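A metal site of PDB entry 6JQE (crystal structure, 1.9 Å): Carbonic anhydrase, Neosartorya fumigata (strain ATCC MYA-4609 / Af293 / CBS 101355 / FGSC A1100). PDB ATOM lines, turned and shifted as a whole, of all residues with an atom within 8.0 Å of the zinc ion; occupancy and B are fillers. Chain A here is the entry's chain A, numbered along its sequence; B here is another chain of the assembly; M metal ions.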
ATOM      1  N   GLY A  25     -22.036   0.389  13.869  1.00  0.00           N
ATOM      2  CA  GLY A  25     -21.180   1.179  14.749  1.00  0.00           C
ATOM      3  C   GLY A  25     -20.551   2.322  14.018  1.00  0.00           C
ATOM      4  O   GLY A  25     -20.702   2.401  12.764  1.00  0.00           O
ATOM      5  N   CYS A  26     -19.796   3.150  14.734  1.00  0.00           N
ATOM      6  CA  CYS A  26     -19.118   4.320  14.143  1.00  0.00           C
ATOM      7  C   CYS A  26     -17.656   3.998  13.762  1.00  0.00           C
ATOM      8  O   CYS A  26     -16.945   3.341  14.527  1.00  0.00           O
ATOM      9  CB  CYS A  26     -19.217   5.501  15.101  1.00  0.00           C
ATOM     10  SG  CYS A  26     -18.514   6.953  14.303  1.00  0.00           S
ATOM     11  N   SER A  27     -17.211   4.560  12.636  1.00  0.00           N
ATOM     12  CA  SER A  27     -15.853   4.508  12.067  1.00  0.00           C
ATOM     13  C   SER A  27     -14.762   5.011  13.042  1.00  0.00           C
ATOM     14  O   SER A  27     -13.659   4.485  12.941  1.00  0.00           O
ATOM     15  CB  SER A  27     -15.805   5.274  10.782  1.00  0.00           C
ATOM     16  OG  SER A  27     -16.605   4.640   9.827  1.00  0.00           O
ATOM     17  N   ASP A  28     -15.045   5.983  13.919  1.00  0.00           N
ATOM     18  CA  ASP A  28     -14.033   6.493  14.877  1.00  0.00           C
ATOM     19  C   ASP A  28     -14.225   5.871  16.261  1.00  0.00           C
ATOM     20  O   ASP A  28     -13.586   6.396  17.228  1.00  0.00           O
ATOM     21  CB  ASP A  28     -13.982   8.032  14.908  1.00  0.00           C
ATOM     22  CG  ASP A  28     -15.195   8.735  15.523  1.00  0.00           C
ATOM     23  OD1 ASP A  28     -15.916   8.111  16.328  1.00  0.00           O
ATOM     24  OD2 ASP A  28     -15.390   9.911  15.313  1.00  0.00           O
ATOM     25  N   SER A  29     -15.042   4.807  16.385  1.00  0.00           N
ATOM     26  CA  SER A  29     -15.078   3.922  17.571  1.00  0.00           C
ATOM     27  C   SER A  29     -14.266   2.636  17.336  1.00  0.00           C
ATOM     28  O   SER A  29     -14.352   2.083  16.250  1.00  0.00           O
ATOM     29  CB  SER A  29     -16.512   3.579  17.920  1.00  0.00           C
ATOM     30  OG  SER A  29     -16.562   2.739  19.051  1.00  0.00           O
ATOM     31  N   GLY A  30     -13.583   2.128  18.367  1.00  0.00           N
ATOM     32  CA  GLY A  30     -12.723   0.920  18.290  1.00  0.00           C
ATOM     33  C   GLY A  30     -13.476  -0.398  18.486  1.00  0.00           C
ATOM     34  O   GLY A  30     -14.688  -0.408  18.837  1.00  0.00           O
ATOM     35  N   GLU A  33     -15.560  -1.535  21.782  1.00  0.00           N
ATOM     36  CA  GLU A  33     -17.036  -1.457  21.778  1.00  0.00           C
ATOM     37  C   GLU A  33     -17.646  -2.871  21.781  1.00  0.00           C
ATOM     38  O   GLU A  33     -18.566  -3.115  22.593  1.00  0.00           O
ATOM     39  CB  GLU A  33     -17.377  -0.631  20.549  1.00  0.00           C
ATOM     40  CG  GLU A  33     -18.768  -0.746  20.035  1.00  0.00           C
ATOM     41  CD  GLU A  33     -18.984   0.146  18.834  1.00  0.00           C
ATOM     42  OE1 GLU A  33     -18.632   1.351  18.904  1.00  0.00           O
ATOM     43  OE2 GLU A  33     -19.545  -0.356  17.852  1.00  0.00           O
ATOM     44  N   ARG A  48     -19.776  -0.595   9.737  1.00  0.00           N
ATOM     45  CA  ARG A  48     -19.132   0.496  10.508  1.00  0.00           C
ATOM     46  C   ARG A  48     -18.976   1.698   9.584  1.00  0.00           C
ATOM     47  O   ARG A  48     -18.260   1.567   8.542  1.00  0.00           O
ATOM     48  CB  ARG A  48     -17.843   0.013  11.176  1.00  0.00           C
ATOM     49  CG  ARG A  48     -17.315   0.987  12.225  1.00  0.00           C
ATOM     50  CD  ARG A  48     -16.216   0.375  13.081  1.00  0.00           C
ATOM     51  NE  ARG A  48     -16.715  -0.681  13.944  1.00  0.00           N
ATOM     52  CZ  ARG A  48     -17.356  -0.525  15.106  1.00  0.00           C
ATOM     53  NH1 ARG A  48     -17.616   0.681  15.600  1.00  0.00           N
ATOM     54  NH2 ARG A  48     -17.732  -1.586  15.799  1.00  0.00           N
ATOM     55  N   SER A  49     -19.630   2.802   9.953  1.00  0.00           N
ATOM     56  CA  SER A  49     -19.933   3.934   9.056  1.00  0.00           C
ATOM     57  C   SER A  49     -19.789   5.252   9.813  1.00  0.00           C
ATOM     58  O   SER A  49     -19.672   5.217  11.054  1.00  0.00           O
ATOM     59  CB  SER A  49     -21.349   3.785   8.530  1.00  0.00           C
ATOM     60  OG  SER A  49     -22.283   3.818   9.636  1.00  0.00           O
ATOM     61  N   LEU A  50     -19.949   6.364   9.091  1.00  0.00           N
ATOM     62  CA  LEU A  50     -19.914   7.730   9.650  1.00  0.00           C
ATOM     63  C   LEU A  50     -21.054   7.876  10.675  1.00  0.00           C
ATOM     64  O   LEU A  50     -22.243   7.801  10.293  1.00  0.00           O
ATOM     65  CB  LEU A  50     -20.059   8.722   8.510  1.00  0.00           C
ATOM     66  CG  LEU A  50     -18.911   8.793   7.510  1.00  0.00           C
ATOM     67  CD1 LEU A  50     -19.188   9.887   6.479  1.00  0.00           C
ATOM     68  CD2 LEU A  50     -17.579   9.071   8.206  1.00  0.00           C
ATOM     69  N   GLY A  51     -20.674   8.085  11.931  1.00  0.00           N
ATOM     70  CA  GLY A  51     -21.602   8.399  13.029  1.00  0.00           C
ATOM     71  C   GLY A  51     -22.612   7.293  13.312  1.00  0.00           C
ATOM     72  O   GLY A  51     -23.698   7.629  13.811  1.00  0.00           O
ATOM     73  N   ASN A  52     -22.280   6.027  13.047  1.00  0.00           N
ATOM     74  CA  ASN A  52     -23.181   4.877  13.268  1.00  0.00           C
ATOM     75  C   ASN A  52     -24.553   5.204  12.664  1.00  0.00           C
ATOM     76  O   ASN A  52     -25.578   4.916  13.272  1.00  0.00           O
ATOM     77  CB  ASN A  52     -23.255   4.414  14.743  1.00  0.00           C
ATOM     78  CG  ASN A  52     -23.402   5.512  15.770  1.00  0.00           C
ATOM     79  OD1 ASN A  52     -22.401   6.037  16.231  1.00  0.00           O
ATOM     80  ND2 ASN A  52     -24.615   5.812  16.208  1.00  0.00           N
ATOM     81  N   CYS A  79     -25.092   1.065  17.758  1.00  0.00           N
ATOM     82  CA  CYS A  79     -24.180   1.381  18.868  1.00  0.00           C
ATOM     83  C   CYS A  79     -23.499   2.741  18.607  1.00  0.00           C
ATOM     84  O   CYS A  79     -22.696   2.882  17.652  1.00  0.00           O
ATOM     85  CB  CYS A  79     -23.172   0.266  19.050  1.00  0.00           C
ATOM     86  SG  CYS A  79     -22.189   0.544  20.551  1.00  0.00           S
ATOM     87  N   GLY A  80     -23.854   3.737  19.402  1.00  0.00           N
ATOM     88  CA  GLY A  80     -23.140   5.025  19.434  1.00  0.00           C
ATOM     89  C   GLY A  80     -22.049   4.939  20.497  1.00  0.00           C
ATOM     90  O   GLY A  80     -21.977   3.927  21.187  1.00  0.00           O
ATOM     91  N   HIS A  81     -21.204   5.958  20.626  1.00  0.00           N
ATOM     92  CA  HIS A  81     -20.105   5.930  21.620  1.00  0.00           C
ATOM     93  C   HIS A  81     -19.795   7.369  22.079  1.00  0.00           C
ATOM     94  O   HIS A  81     -19.638   8.266  21.213  1.00  0.00           O
ATOM     95  CB  HIS A  81     -18.883   5.209  21.019  1.00  0.00           C
ATOM     96  CG  HIS A  81     -18.276   5.920  19.845  1.00  0.00           C
ATOM     97  ND1 HIS A  81     -16.967   6.351  19.866  1.00  0.00           N
ATOM     98  CD2 HIS A  81     -18.785   6.332  18.654  1.00  0.00           C
ATOM     99  CE1 HIS A  81     -16.682   6.988  18.745  1.00  0.00           C
ATOM    100  NE2 HIS A  81     -17.795   6.984  17.958  1.00  0.00           N
ATOM    101  N   TYR A  82     -19.649   7.551  23.381  1.00  0.00           N
ATOM    102  CA  TYR A  82     -19.251   8.834  24.005  1.00  0.00           C
ATOM    103  C   TYR A  82     -17.848   9.220  23.506  1.00  0.00           C
ATOM    104  O   TYR A  82     -16.980   8.333  23.384  1.00  0.00           O
ATOM    105  CB  TYR A  82     -19.339   8.743  25.527  1.00  0.00           C
ATOM    106  CG  TYR A  82     -20.735   8.532  26.053  1.00  0.00           C
ATOM    107  CD1 TYR A  82     -21.770   9.351  25.644  1.00  0.00           C
ATOM    108  CD2 TYR A  82     -21.012   7.538  26.977  1.00  0.00           C
ATOM    109  CE1 TYR A  82     -23.051   9.184  26.144  1.00  0.00           C
ATOM    110  CE2 TYR A  82     -22.296   7.351  27.451  1.00  0.00           C
ATOM    111  CZ  TYR A  82     -23.326   8.163  27.031  1.00  0.00           C
ATOM    112  OH  TYR A  82     -24.596   7.986  27.507  1.00  0.00           O
ATOM    113  N   GLY A  83     -17.651  10.503  23.193  1.00  0.00           N
ATOM    114  CA  GLY A  83     -16.377  11.013  22.647  1.00  0.00           C
ATOM    115  C   GLY A  83     -16.325  10.912  21.125  1.00  0.00           C
ATOM    116  O   GLY A  83     -15.282  11.261  20.512  1.00  0.00           O
ATOM    117  N   CYS A  84     -17.437  10.503  20.499  1.00  0.00           N
ATOM    118  CA  CYS A  84     -17.563  10.452  19.020  1.00  0.00           C
ATOM    119  C   CYS A  84     -17.219  11.849  18.462  1.00  0.00           C
ATOM    120  O   CYS A  84     -17.742  12.858  19.004  1.00  0.00           O
ATOM    121  CB  CYS A  84     -18.973  10.016  18.624  1.00  0.00           C
ATOM    122  SG  CYS A  84     -19.287   9.970  16.834  1.00  0.00           S
ATOM    123  N   HIS A  85     -16.371  11.946  17.448  1.00  0.00           N
ATOM    124  CA  HIS A  85     -15.979  13.230  16.797  1.00  0.00           C
ATOM    125  C   HIS A  85     -17.031  13.649  15.786  1.00  0.00           C
ATOM    126  O   HIS A  85     -17.087  14.839  15.481  1.00  0.00           O
ATOM    127  CB  HIS A  85     -14.580  13.090  16.164  1.00  0.00           C
ATOM    128  CG  HIS A  85     -13.513  12.840  17.168  1.00  0.00           C
ATOM    129  ND1 HIS A  85     -13.166  13.790  18.105  1.00  0.00           N
ATOM    130  CD2 HIS A  85     -12.758  11.757  17.451  1.00  0.00           C
ATOM    131  CE1 HIS A  85     -12.232  13.310  18.891  1.00  0.00           C
ATOM    132  NE2 HIS A  85     -11.966  12.077  18.517  1.00  0.00           N
ATOM    133  N   ILE A  86     -17.848  12.724  15.287  1.00  0.00           N
ATOM    134  CA  ILE A  86     -18.819  13.001  14.179  1.00  0.00           C
ATOM    135  C   ILE A  86     -20.143  13.448  14.790  1.00  0.00           C
ATOM    136  O   ILE A  86     -20.651  14.489  14.355  1.00  0.00           O
ATOM    137  CB  ILE A  86     -18.933  11.763  13.257  1.00  0.00           C
ATOM    138  CG1 ILE A  86     -17.613  11.489  12.532  1.00  0.00           C
ATOM    139  CG2 ILE A  86     -20.092  11.914  12.267  1.00  0.00           C
ATOM    140  CD1 ILE A  86     -17.473  10.063  12.036  1.00  0.00           C
ATOM    141  N   ALA A  87     -20.714  12.706  15.745  1.00  0.00           N
ATOM    142  CA  ALA A  87     -21.915  13.100  16.496  1.00  0.00           C
ATOM    143  C   ALA A  87     -21.494  14.008  17.655  1.00  0.00           C
ATOM    144  O   ALA A  87     -21.603  13.580  18.828  1.00  0.00           O
ATOM    145  CB  ALA A  87     -22.711  11.923  16.989  1.00  0.00           C
ATOM    146  N   SER A  88     -21.028  15.210  17.342  1.00  0.00           N
ATOM    147  CA  SER A  88     -20.573  16.170  18.380  1.00  0.00           C
ATOM    148  C   SER A  88     -20.776  17.605  17.915  1.00  0.00           C
ATOM    149  O   SER A  88     -20.926  17.823  16.703  1.00  0.00           O
ATOM    150  CB  SER A  88     -19.136  15.947  18.731  1.00  0.00           C
ATOM    151  OG  SER A  88     -18.319  16.631  17.822  1.00  0.00           O
ATOM    152  N   VAL A 127     -24.826  12.199  21.090  1.00  0.00           N
ATOM    153  CA  VAL A 127     -24.588  10.753  20.800  1.00  0.00           C
ATOM    154  C   VAL A 127     -25.878   9.965  21.064  1.00  0.00           C
ATOM    155  O   VAL A 127     -26.275   9.124  20.210  1.00  0.00           O
ATOM    156  CB  VAL A 127     -23.407  10.207  21.612  1.00  0.00           C
ATOM    157  CG1 VAL A 127     -23.343   8.710  21.521  1.00  0.00           C
ATOM    158  CG2 VAL A 127     -22.104  10.861  21.163  1.00  0.00           C
ATOM    159  N   ASN A 130     -28.717  10.762  18.648  1.00  0.00           N
ATOM    160  CA  ASN A 130     -28.423  10.201  17.311  1.00  0.00           C
ATOM    161  C   ASN A 130     -28.815   8.714  17.285  1.00  0.00           C
ATOM    162  O   ASN A 130     -29.465   8.318  16.335  1.00  0.00           O
ATOM    163  CB  ASN A 130     -26.968  10.418  16.906  1.00  0.00           C
ATOM    164  CG  ASN A 130     -26.668   9.891  15.521  1.00  0.00           C
ATOM    165  OD1 ASN A 130     -27.403  10.165  14.590  1.00  0.00           O
ATOM    166  ND2 ASN A 130     -25.629   9.119  15.381  1.00  0.00           N
ATOM    167  N   PHE B  45      -9.165   4.459  11.679  1.00  0.00           N
ATOM    168  CA  PHE B  45     -10.522   4.911  11.252  1.00  0.00           C
ATOM    169  C   PHE B  45     -11.096   3.805  10.368  1.00  0.00           C
ATOM    170  O   PHE B  45     -10.544   3.591   9.295  1.00  0.00           O
ATOM    171  CB  PHE B  45     -10.427   6.235  10.514  1.00  0.00           C
ATOM    172  CG  PHE B  45     -11.750   6.889  10.219  1.00  0.00           C
ATOM    173  CD1 PHE B  45     -12.471   7.494  11.237  1.00  0.00           C
ATOM    174  CD2 PHE B  45     -12.268   6.900   8.931  1.00  0.00           C
ATOM    175  CE1 PHE B  45     -13.671   8.120  10.982  1.00  0.00           C
ATOM    176  CE2 PHE B  45     -13.464   7.544   8.668  1.00  0.00           C
ATOM    177  CZ  PHE B  45     -14.180   8.128   9.691  1.00  0.00           C
ATOM    178  N   TYR B  66     -14.438  12.581   4.187  1.00  0.00           N
ATOM    179  CA  TYR B  66     -14.241  12.957   5.607  1.00  0.00           C
ATOM    180  C   TYR B  66     -12.832  12.527   6.005  1.00  0.00           C
ATOM    181  O   TYR B  66     -12.125  13.297   6.691  1.00  0.00           O
ATOM    182  CB  TYR B  66     -15.318  12.334   6.496  1.00  0.00           C
ATOM    183  CG  TYR B  66     -15.124  12.570   7.976  1.00  0.00           C
ATOM    184  CD1 TYR B  66     -15.544  13.743   8.590  1.00  0.00           C
ATOM    185  CD2 TYR B  66     -14.509  11.636   8.772  1.00  0.00           C
ATOM    186  CE1 TYR B  66     -15.386  13.947   9.948  1.00  0.00           C
ATOM    187  CE2 TYR B  66     -14.320  11.834  10.131  1.00  0.00           C
ATOM    188  CZ  TYR B  66     -14.781  12.989  10.734  1.00  0.00           C
ATOM    189  OH  TYR B  66     -14.591  13.187  12.092  1.00  0.00           O
HETATM  190 ZN    ZN M   1     -18.026   8.030  16.327  1.00  0.00          ZN
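NE2 of His 81 is bound to the zinc ion, 2.0 Å away.
The zinc ion is bound by OD1 of Asp 28.
SG of Cys 26 is bound to the zinc ion.
SG of Cys 84 is bound to the zinc ion.
The backbone NH of Ile 86 lies close to the side-chain sulfur of Cys 84 (3.5 Å).
SG of Cys 84 lies close to N of Ala 87, at 3.3 Å.
N of Gly 51 sits close to SG of Cys 26, 3.4 Å away.
The backbone NH (N) of His 85 sits at hydrogen-bond distance from the side-chain carboxylate (OD2) of Asp 28 (3.1 Å).
NH1 of Arg 48 sits at hydrogen-bond distance from O of Cys 26 (2.9 Å).
Within 4 Å of the zinc ion: Cys 26, Asp 28, His 81 and Cys 84.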
